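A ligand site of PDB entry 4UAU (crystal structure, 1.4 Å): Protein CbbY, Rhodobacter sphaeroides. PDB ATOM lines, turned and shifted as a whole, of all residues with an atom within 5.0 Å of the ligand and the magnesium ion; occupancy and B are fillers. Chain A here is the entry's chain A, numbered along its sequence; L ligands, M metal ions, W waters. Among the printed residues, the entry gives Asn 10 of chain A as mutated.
The backbone NH of Asn 10 lies within hydrogen-bond range of an oxygen (O8) of the ligand. The side-chain amide nitrogen (ND2) of Asn 10 is in hydrogen-bond range of an oxygen (O1) of the ligand, at 2.9 Å. OG1 of Thr 115 sits at hydrogen-bond distance from O8 of the ligand. O4 of the ligand is in hydrogen-bond range of OE2 of Glu 17 (2.6 Å). NE2 of His 75 sits at hydrogen-bond distance from O10 of the ligand (2.7 Å). The backbone NH of Gly 51 lies within hydrogen-bond range of an oxygen (O11) of the ligand, 2.7 Å away. O9 of the ligand sits at hydrogen-bond distance from N of Ser 118, 2.9 Å away. OG of Ser 118 sits at hydrogen-bond distance from O9 of the ligand (2.8 Å). The backbone NH of Thr 116 lies within hydrogen-bond range of an oxygen (O6) of the ligand (2.9 Å). O6 of the ligand lies within hydrogen-bond range of OG1 of Thr 116. The backbone NH of Gly 50 sits at hydrogen-bond distance from an oxygen (O3) of the ligand (2.8 Å). The side-chain amino group (NZ) of Lys 78 is in salt-bridge range of an oxygen (O10) of the ligand (2.8 Å). The guanidinium group (NH1) of Arg 54 sits at hydrogen-bond distance from an oxygen (O4) of the ligand (2.9 Å). OG1 of Thr 117 sits at hydrogen-bond distance from O5 of the ligand (2.9 Å). The side-chain amide nitrogen (ND2) of Asn 121 is in hydrogen-bond range of an oxygen (O9) of the ligand (3.1 Å). An oxygen (O8) of the ligand sits at hydrogen-bond distance from the backbone NH (N) of Val 9, at 3.4 Å. The side-chain amino group (NZ) of Lys 151 is in salt-bridge range of an oxygen (O6) of the ligand, at 3.5 Å.
The backbone NH (N) of Asp 176 lies within hydrogen-bond range of the side-chain hydroxyl (OG1) of Thr 12 (3.2 Å). OG1 of Thr 117 sits at hydrogen-bond distance from ND2 of Asn 10 (3.0 Å). The backbone NH (N) of Thr 117 sits at hydrogen-bond distance from the side-chain hydroxyl (OG1) of Thr 115 (3.1 Å). The side-chain hydroxyl (OH) of Tyr 42 lies within hydrogen-bond range of the side-chain carboxylate (OE1) of Glu 17 (2.7 Å). O of His 75 sits at hydrogen-bond distance from OG1 of Thr 79 (3.0 Å). The side-chain amino group (NZ) of Lys 78 lies within hydrogen-bond range of a ring nitrogen (ND1) of His 20 (2.9 Å). The backbone carbonyl oxygen (O) of Thr 48 sits at hydrogen-bond distance from the guanidinium group (NH2) of Arg 54, 2.9 Å away. The side-chain hydroxyl of Thr 117 sits at hydrogen-bond distance from the side-chain amide nitrogen of Asn 121.
CE1 of His 20 touches O5 of the ligand (3.6 Å). Phe 24 touches the ligand (CZ to O10, 3.8 Å). Leu 46 touches the ligand (CD2 to O4, 3.8 Å). CA of Thr 49 touches O2 of the ligand (3.3 Å).
Within 4 Å of the magnesium ion: Asp 8, Asn 10 and Asp 176. The nearest printed residue that does not touch the magnesium ion is Glu 175 (4.01 Å).
The magnesium ion is bound by an oxygen (O7) of the ligand, the side-chain carboxylate (OD2) of Asp 8, the side-chain carboxylate (OD1) of Asp 176, water W5, water W3 and the backbone carbonyl oxygen (O) of Asn 10. The magnesium ion has six donor atoms within binding distance.
Water W5 lies within hydrogen-bond range of the side-chain carboxylate (OE1) of Glu 175, the side-chain hydroxyl (OG) of Ser 177 and the side-chain carboxylate (OD1) of Asp 8. Water W4 lies within hydrogen-bond range of O11 of the ligand (2.6 Å) and O of Thr 116 (2.8 Å). Water W2 lies within hydrogen-bond range of an oxygen (O9) of the ligand, the side-chain amino group of Lys 78, the side-chain hydroxyl of Thr 79, the side-chain amide nitrogen of Asn 121, the side-chain hydroxyl of Ser 118 and a ring nitrogen (NE2) of His 75. Water W1 lies within hydrogen-bond range of the backbone carbonyl oxygen (O) of Leu 46 and an oxygen (O2) of the ligand.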
ATOM      1  N   ASP A   8       5.157   1.361 -12.051  1.00  0.00           N
ATOM      2  CA  ASP A   8       6.006   1.136 -10.899  1.00  0.00           C
ATOM      3  C   ASP A   8       5.917   2.339  -9.942  1.00  0.00           C
ATOM      4  O   ASP A   8       5.465   3.429 -10.339  1.00  0.00           O
ATOM      5  CB  ASP A   8       7.445   0.909 -11.381  1.00  0.00           C
ATOM      6  CG  ASP A   8       8.391   0.693 -10.251  1.00  0.00           C
ATOM      7  OD1 ASP A   8       8.095  -0.230  -9.445  1.00  0.00           O
ATOM      8  OD2 ASP A   8       9.367   1.444 -10.150  1.00  0.00           O
ATOM      9  N   VAL A   9       6.359   2.167  -8.696  1.00  0.00           N
ATOM     10  CA  VAL A   9       6.327   3.280  -7.733  1.00  0.00           C
ATOM     11  C   VAL A   9       7.727   3.851  -7.493  1.00  0.00           C
ATOM     12  O   VAL A   9       8.035   4.943  -7.975  1.00  0.00           O
ATOM     13  CB  VAL A   9       5.657   2.890  -6.397  1.00  0.00           C
ATOM     14  CG1 VAL A   9       5.783   3.996  -5.331  1.00  0.00           C
ATOM     15  CG2 VAL A   9       4.192   2.605  -6.636  1.00  0.00           C
ATOM     16  N   ASN A  10       8.605   3.088  -6.825  1.00  0.00           N
ATOM     17  CA  ASN A  10       9.881   3.657  -6.399  1.00  0.00           C
ATOM     18  C   ASN A  10      10.818   3.890  -7.556  1.00  0.00           C
ATOM     19  O   ASN A  10      11.141   2.952  -8.308  1.00  0.00           O
ATOM     20  CB  ASN A  10      10.499   2.802  -5.300  1.00  0.00           C
ATOM     21  CG  ASN A  10       9.657   2.822  -4.027  1.00  0.00           C
ATOM     22  OD1 ASN A  10       9.357   3.899  -3.490  1.00  0.00           O
ATOM     23  ND2 ASN A  10       9.229   1.658  -3.581  1.00  0.00           N
ATOM     24  N   GLY A  11      11.235   5.139  -7.743  1.00  0.00           N
ATOM     25  CA  GLY A  11      12.088   5.471  -8.869  1.00  0.00           C
ATOM     26  C   GLY A  11      11.333   5.822 -10.132  1.00  0.00           C
ATOM     27  O   GLY A  11      11.942   6.281 -11.102  1.00  0.00           O
ATOM     28  N   THR A  12      10.023   5.580 -10.148  1.00  0.00           N
ATOM     29  CA  THR A  12       9.199   5.779 -11.353  1.00  0.00           C
ATOM     30  C   THR A  12       8.216   6.931 -11.151  1.00  0.00           C
ATOM     31  O   THR A  12       8.309   7.944 -11.869  1.00  0.00           O
ATOM     32  CB  THR A  12       8.514   4.452 -11.733  1.00  0.00           C
ATOM     33  OG1 THR A  12       9.530   3.483 -12.064  1.00  0.00           O
ATOM     34  CG2 THR A  12       7.648   4.624 -12.920  1.00  0.00           C
ATOM     35  N   GLU A  17      14.216   6.518  -3.231  1.00  0.00           N
ATOM     36  CA  GLU A  17      15.088   5.544  -2.542  1.00  0.00           C
ATOM     37  C   GLU A  17      15.985   6.141  -1.474  1.00  0.00           C
ATOM     38  O   GLU A  17      16.284   5.477  -0.495  1.00  0.00           O
ATOM     39  CB  GLU A  17      15.874   4.669  -3.529  1.00  0.00           C
ATOM     40  CG  GLU A  17      14.999   3.572  -4.149  1.00  0.00           C
ATOM     41  CD  GLU A  17      14.452   2.544  -3.150  1.00  0.00           C
ATOM     42  OE1 GLU A  17      14.869   2.533  -1.958  1.00  0.00           O
ATOM     43  OE2 GLU A  17      13.610   1.733  -3.573  1.00  0.00           O
ATOM     44  N   HIS A  20      13.780   6.054   1.465  1.00  0.00           N
ATOM     45  CA  HIS A  20      13.789   4.685   1.977  1.00  0.00           C
ATOM     46  C   HIS A  20      15.053   4.399   2.778  1.00  0.00           C
ATOM     47  O   HIS A  20      14.977   3.833   3.872  1.00  0.00           O
ATOM     48  CB  HIS A  20      13.597   3.620   0.870  1.00  0.00           C
ATOM     49  CG  HIS A  20      12.204   3.555   0.329  1.00  0.00           C
ATOM     50  ND1 HIS A  20      11.155   3.022   1.031  1.00  0.00           N
ATOM     51  CD2 HIS A  20      11.704   3.910  -0.885  1.00  0.00           C
ATOM     52  CE1 HIS A  20      10.068   3.064   0.301  1.00  0.00           C
ATOM     53  NE2 HIS A  20      10.369   3.605  -0.864  1.00  0.00           N
ATOM     54  N   PHE A  24      15.287   3.241   6.696  1.00  0.00           N
ATOM     55  CA  PHE A  24      15.990   2.029   7.158  1.00  0.00           C
ATOM     56  C   PHE A  24      16.992   2.415   8.241  1.00  0.00           C
ATOM     57  O   PHE A  24      16.981   1.853   9.348  1.00  0.00           O
ATOM     58  CB  PHE A  24      16.724   1.305   6.013  1.00  0.00           C
ATOM     59  CG  PHE A  24      15.833   0.424   5.143  1.00  0.00           C
ATOM     60  CD1 PHE A  24      15.303  -0.762   5.639  1.00  0.00           C
ATOM     61  CD2 PHE A  24      15.569   0.780   3.802  1.00  0.00           C
ATOM     62  CE1 PHE A  24      14.501  -1.574   4.831  1.00  0.00           C
ATOM     63  CE2 PHE A  24      14.776  -0.052   2.997  1.00  0.00           C
ATOM     64  CZ  PHE A  24      14.238  -1.221   3.530  1.00  0.00           C
ATOM     65  N   TYR A  42      23.755   0.390  -0.291  1.00  0.00           N
ATOM     66  CA  TYR A  42      22.356   0.378  -0.699  1.00  0.00           C
ATOM     67  C   TYR A  42      22.162   0.084  -2.195  1.00  0.00           C
ATOM     68  O   TYR A  42      21.232  -0.640  -2.558  1.00  0.00           O
ATOM     69  CB  TYR A  42      21.678   1.698  -0.278  1.00  0.00           C
ATOM     70  CG  TYR A  42      20.188   1.566  -0.172  1.00  0.00           C
ATOM     71  CD1 TYR A  42      19.602   0.639   0.694  1.00  0.00           C
ATOM     72  CD2 TYR A  42      19.355   2.419  -0.925  1.00  0.00           C
ATOM     73  CE1 TYR A  42      18.174   0.541   0.791  1.00  0.00           C
ATOM     74  CE2 TYR A  42      17.977   2.332  -0.821  1.00  0.00           C
ATOM     75  CZ  TYR A  42      17.391   1.384   0.007  1.00  0.00           C
ATOM     76  OH  TYR A  42      16.016   1.313   0.105  1.00  0.00           O
ATOM     77  N   LEU A  46      19.728  -2.912  -3.320  1.00  0.00           N
ATOM     78  CA  LEU A  46      18.532  -2.605  -4.113  1.00  0.00           C
ATOM     79  C   LEU A  46      18.235  -3.617  -5.222  1.00  0.00           C
ATOM     80  O   LEU A  46      17.111  -3.639  -5.735  1.00  0.00           O
ATOM     81  CB  LEU A  46      18.629  -1.201  -4.703  1.00  0.00           C
ATOM     82  CG  LEU A  46      18.224  -0.103  -3.734  1.00  0.00           C
ATOM     83  CD1 LEU A  46      18.644   1.261  -4.318  1.00  0.00           C
ATOM     84  CD2 LEU A  46      16.719  -0.119  -3.453  1.00  0.00           C
ATOM     85  N   THR A  48      17.826  -6.652  -4.639  1.00  0.00           N
ATOM     86  CA  THR A  48      16.830  -7.513  -4.001  1.00  0.00           C
ATOM     87  C   THR A  48      15.635  -6.655  -3.679  1.00  0.00           C
ATOM     88  O   THR A  48      15.781  -5.715  -2.898  1.00  0.00           O
ATOM     89  CB  THR A  48      17.384  -8.091  -2.684  1.00  0.00           C
ATOM     90  OG1 THR A  48      18.462  -8.984  -3.010  1.00  0.00           O
ATOM     91  CG2 THR A  48      16.305  -8.835  -1.903  1.00  0.00           C
ATOM     92  N   THR A  49      14.476  -6.938  -4.298  1.00  0.00           N
ATOM     93  CA  THR A  49      13.305  -6.104  -4.039  1.00  0.00           C
ATOM     94  C   THR A  49      12.545  -6.581  -2.780  1.00  0.00           C
ATOM     95  O   THR A  49      12.572  -7.781  -2.409  1.00  0.00           O
ATOM     96  CB  THR A  49      12.315  -6.065  -5.227  1.00  0.00           C
ATOM     97  OG1 THR A  49      11.697  -7.351  -5.403  1.00  0.00           O
ATOM     98  CG2 THR A  49      13.052  -5.699  -6.506  1.00  0.00           C
ATOM     99  N   GLY A  50      11.858  -5.627  -2.152  1.00  0.00           N
ATOM    100  CA  GLY A  50      11.143  -5.859  -0.888  1.00  0.00           C
ATOM    101  C   GLY A  50      12.063  -5.600   0.295  1.00  0.00           C
ATOM    102  O   GLY A  50      13.146  -6.157   0.406  1.00  0.00           O
ATOM    103  N   GLY A  51      11.599  -4.786   1.218  1.00  0.00           N
ATOM    104  CA  GLY A  51      12.446  -4.425   2.347  1.00  0.00           C
ATOM    105  C   GLY A  51      12.747  -5.562   3.299  1.00  0.00           C
ATOM    106  O   GLY A  51      13.850  -5.632   3.872  1.00  0.00           O
ATOM    107  N   ARG A  54      15.352  -7.573   1.617  1.00  0.00           N
ATOM    108  CA  ARG A  54      16.625  -6.854   1.604  1.00  0.00           C
ATOM    109  C   ARG A  54      17.313  -6.962   2.951  1.00  0.00           C
ATOM    110  O   ARG A  54      18.523  -7.212   3.011  1.00  0.00           O
ATOM    111  CB  ARG A  54      16.378  -5.393   1.280  1.00  0.00           C
ATOM    112  CG  ARG A  54      17.660  -4.598   1.014  1.00  0.00           C
ATOM    113  CD  ARG A  54      17.379  -3.175   0.431  1.00  0.00           C
ATOM    114  NE  ARG A  54      16.618  -3.326  -0.795  1.00  0.00           N
ATOM    115  CZ  ARG A  54      15.528  -2.662  -1.136  1.00  0.00           C
ATOM    116  NH1 ARG A  54      15.121  -1.597  -0.461  1.00  0.00           N
ATOM    117  NH2 ARG A  54      14.878  -3.080  -2.226  1.00  0.00           N
ATOM    118  N   HIS A  75      10.879  -4.280   9.727  1.00  0.00           N
ATOM    119  CA  HIS A  75      10.378  -3.678   8.515  1.00  0.00           C
ATOM    120  C   HIS A  75       9.088  -2.896   8.722  1.00  0.00           C
ATOM    121  O   HIS A  75       8.858  -1.865   8.118  1.00  0.00           O
ATOM    122  CB  HIS A  75      10.173  -4.693   7.414  1.00  0.00           C
ATOM    123  CG  HIS A  75       9.923  -4.054   6.093  1.00  0.00           C
ATOM    124  ND1 HIS A  75       8.733  -4.187   5.408  1.00  0.00           N
ATOM    125  CD2 HIS A  75      10.690  -3.202   5.357  1.00  0.00           C
ATOM    126  CE1 HIS A  75       8.790  -3.471   4.298  1.00  0.00           C
ATOM    127  NE2 HIS A  75       9.961  -2.860   4.246  1.00  0.00           N
ATOM    128  N   LYS A  78      10.169   0.387   9.997  1.00  0.00           N
ATOM    129  CA  LYS A  78      10.740   1.148   8.893  1.00  0.00           C
ATOM    130  C   LYS A  78       9.630   1.731   8.013  1.00  0.00           C
ATOM    131  O   LYS A  78       9.697   2.900   7.567  1.00  0.00           O
ATOM    132  CB  LYS A  78      11.710   0.280   8.104  1.00  0.00           C
ATOM    133  CG  LYS A  78      12.231   0.966   6.815  1.00  0.00           C
ATOM    134  CD  LYS A  78      11.374   0.650   5.585  1.00  0.00           C
ATOM    135  CE  LYS A  78      11.761   1.534   4.439  1.00  0.00           C
ATOM    136  NZ  LYS A  78      10.919   1.187   3.250  1.00  0.00           N
ATOM    137  N   THR A  79       8.589   0.933   7.759  1.00  0.00           N
ATOM    138  CA  THR A  79       7.440   1.436   7.008  1.00  0.00           C
ATOM    139  C   THR A  79       6.761   2.617   7.704  1.00  0.00           C
ATOM    140  O   THR A  79       6.487   3.647   7.074  1.00  0.00           O
ATOM    141  CB  THR A  79       6.430   0.311   6.725  1.00  0.00           C
ATOM    142  OG1 THR A  79       7.093  -0.704   5.976  1.00  0.00           O
ATOM    143  CG2 THR A  79       5.220   0.822   5.964  1.00  0.00           C
ATOM    144  N   THR A 115       3.933  -2.700  -7.775  1.00  0.00           N
ATOM    145  CA  THR A 115       5.121  -2.320  -6.993  1.00  0.00           C
ATOM    146  C   THR A 115       5.473  -3.379  -5.993  1.00  0.00           C
ATOM    147  O   THR A 115       4.604  -4.133  -5.530  1.00  0.00           O
ATOM    148  CB  THR A 115       4.887  -0.956  -6.284  1.00  0.00           C
ATOM    149  OG1 THR A 115       6.059  -0.588  -5.556  1.00  0.00           O
ATOM    150  CG2 THR A 115       3.708  -1.013  -5.324  1.00  0.00           C
ATOM    151  N   THR A 116       6.754  -3.444  -5.666  1.00  0.00           N
ATOM    152  CA  THR A 116       7.268  -4.315  -4.600  1.00  0.00           C
ATOM    153  C   THR A 116       7.126  -3.683  -3.228  1.00  0.00           C
ATOM    154  O   THR A 116       7.281  -4.374  -2.215  1.00  0.00           O
ATOM    155  CB  THR A 116       8.765  -4.686  -4.806  1.00  0.00           C
ATOM    156  OG1 THR A 116       9.568  -3.499  -4.717  1.00  0.00           O
ATOM    157  CG2 THR A 116       8.980  -5.349  -6.186  1.00  0.00           C
ATOM    158  N   THR A 117       6.831  -2.381  -3.193  1.00  0.00           N
ATOM    159  CA  THR A 117       6.825  -1.617  -1.927  1.00  0.00           C
ATOM    160  C   THR A 117       5.585  -1.885  -1.086  1.00  0.00           C
ATOM    161  O   THR A 117       4.531  -2.315  -1.616  1.00  0.00           O
ATOM    162  CB  THR A 117       6.980  -0.089  -2.266  1.00  0.00           C
ATOM    163  OG1 THR A 117       7.652   0.598  -1.204  1.00  0.00           O
ATOM    164  CG2 THR A 117       5.650   0.628  -2.506  1.00  0.00           C
ATOM    165  N   SER A 118       5.706  -1.599   0.207  1.00  0.00           N
ATOM    166  CA  SER A 118       4.585  -1.751   1.151  1.00  0.00           C
ATOM    167  C   SER A 118       3.420  -0.846   0.788  1.00  0.00           C
ATOM    168  O   SER A 118       3.613   0.316   0.438  1.00  0.00           O
ATOM    169  CB  SER A 118       5.063  -1.420   2.555  1.00  0.00           C
ATOM    170  OG  SER A 118       6.169  -2.227   2.861  1.00  0.00           O
ATOM    171  N   ASN A 121       3.101   2.822   1.859  1.00  0.00           N
ATOM    172  CA  ASN A 121       3.990   3.742   1.170  1.00  0.00           C
ATOM    173  C   ASN A 121       3.338   4.357  -0.060  1.00  0.00           C
ATOM    174  O   ASN A 121       3.623   5.493  -0.409  1.00  0.00           O
ATOM    175  CB  ASN A 121       5.263   3.022   0.710  1.00  0.00           C
ATOM    176  CG  ASN A 121       6.079   2.482   1.865  1.00  0.00           C
ATOM    177  OD1 ASN A 121       5.909   2.885   3.023  1.00  0.00           O
ATOM    178  ND2 ASN A 121       7.008   1.597   1.540  1.00  0.00           N
ATOM    179  N   LYS A 151       9.215  -8.771  -7.836  1.00  0.00           N
ATOM    180  CA  LYS A 151       9.984  -8.513  -9.068  1.00  0.00           C
ATOM    181  C   LYS A 151      11.417  -8.990  -8.823  1.00  0.00           C
ATOM    182  O   LYS A 151      11.999  -8.724  -7.770  1.00  0.00           O
ATOM    183  CB  LYS A 151       9.948  -7.027  -9.456  1.00  0.00           C
ATOM    184  CG  LYS A 151       8.544  -6.390  -9.488  1.00  0.00           C
ATOM    185  CD  LYS A 151       8.597  -4.966 -10.002  1.00  0.00           C
ATOM    186  CE  LYS A 151       7.301  -4.261  -9.754  1.00  0.00           C
ATOM    187  NZ  LYS A 151       7.501  -2.781  -9.998  1.00  0.00           N
ATOM    188  N   GLU A 175       8.682   1.758 -15.831  1.00  0.00           N
ATOM    189  CA  GLU A 175       9.626   1.191 -14.838  1.00  0.00           C
ATOM    190  C   GLU A 175      10.900   1.996 -14.795  1.00  0.00           C
ATOM    191  O   GLU A 175      11.200   2.780 -15.727  1.00  0.00           O
ATOM    192  CB  GLU A 175       9.966  -0.259 -15.209  1.00  0.00           C
ATOM    193  CG  GLU A 175       8.938  -1.234 -14.686  1.00  0.00           C
ATOM    194  CD  GLU A 175       9.101  -1.503 -13.209  1.00  0.00           C
ATOM    195  OE1 GLU A 175      10.003  -0.907 -12.575  1.00  0.00           O
ATOM    196  OE2 GLU A 175       8.277  -2.281 -12.654  1.00  0.00           O
ATOM    197  N   ASP A 176      11.665   1.784 -13.732  1.00  0.00           N
ATOM    198  CA  ASP A 176      12.964   2.425 -13.563  1.00  0.00           C
ATOM    199  C   ASP A 176      14.126   1.487 -13.399  1.00  0.00           C
ATOM    200  O   ASP A 176      15.266   1.913 -13.440  1.00  0.00           O
ATOM    201  CB  ASP A 176      12.954   3.353 -12.331  1.00  0.00           C
ATOM    202  CG  ASP A 176      12.904   2.553 -11.017  1.00  0.00           C
ATOM    203  OD1 ASP A 176      11.948   1.755 -10.840  1.00  0.00           O
ATOM    204  OD2 ASP A 176      13.843   2.670 -10.185  1.00  0.00           O
ATOM    205  N   SER A 177      13.836   0.209 -13.155  1.00  0.00           N
ATOM    206  CA  SER A 177      14.869  -0.745 -12.777  1.00  0.00           C
ATOM    207  C   SER A 177      14.855  -2.014 -13.634  1.00  0.00           C
ATOM    208  O   SER A 177      13.854  -2.346 -14.258  1.00  0.00           O
ATOM    209  CB  SER A 177      14.743  -1.131 -11.284  1.00  0.00           C
ATOM    210  OG  SER A 177      13.612  -1.959 -11.071  1.00  0.00           O
HETATM  211  C1  LIG L   1      11.442  -1.048  -5.071  1.00  0.00           C
HETATM  212  C2  LIG L   1      11.757  -1.949  -3.880  1.00  0.00           C
HETATM  213  C3  LIG L   1      11.132  -1.739  -2.538  1.00  0.00           C
HETATM  214  C4  LIG L   1      11.705  -0.440  -1.950  1.00  0.00           C
HETATM  215  C5  LIG L   1      11.459  -0.295  -0.459  1.00  0.00           C
HETATM  216  O1  LIG L   1      10.051  -0.614  -5.176  1.00  0.00           O
HETATM  217  O2  LIG L   1      12.608  -2.841  -4.038  1.00  0.00           O
HETATM  218  O3  LIG L   1      11.450  -2.881  -1.737  1.00  0.00           O
HETATM  219  O4  LIG L   1      13.133  -0.428  -2.137  1.00  0.00           O
HETATM  220  O5  LIG L   1      10.088  -0.470  -0.109  1.00  0.00           O
HETATM  221  P1  LIG L   1       9.315  -0.497  -6.640  1.00  0.00           P
HETATM  222  P2  LIG L   1       9.691  -1.533   1.027  1.00  0.00           P
HETATM  223  O6  LIG L   1       8.929  -1.929  -6.935  1.00  0.00           O
HETATM  224  O7  LIG L   1      10.370   0.075  -7.564  1.00  0.00           O
HETATM  225  O8  LIG L   1       8.158   0.444  -6.393  1.00  0.00           O
HETATM  226  O9  LIG L   1       8.295  -1.168   1.418  1.00  0.00           O
HETATM  227  O10 LIG L   1      10.692  -1.392   2.163  1.00  0.00           O
HETATM  228  O11 LIG L   1       9.773  -2.910   0.430  1.00  0.00           O
HETATM  229 MG    MG M   1      11.053   0.938  -9.169  1.00  0.00          MG
HETATM  230  O   HOH W   1      14.746  -2.133  -5.790  1.00  0.00           O
HETATM  231  O   HOH W   2       8.397   0.205   3.728  1.00  0.00           O
HETATM  232  O   HOH W   3      13.103   0.670  -8.463  1.00  0.00           O
HETATM  233  O   HOH W   4       7.954  -4.794   0.451  1.00  0.00           O
HETATM  234  O   HOH W   5      11.210  -0.914 -10.227  1.00  0.00           O
HETATM  235  O   HOH W   6      10.888  -3.033  -8.504  1.00  0.00           O
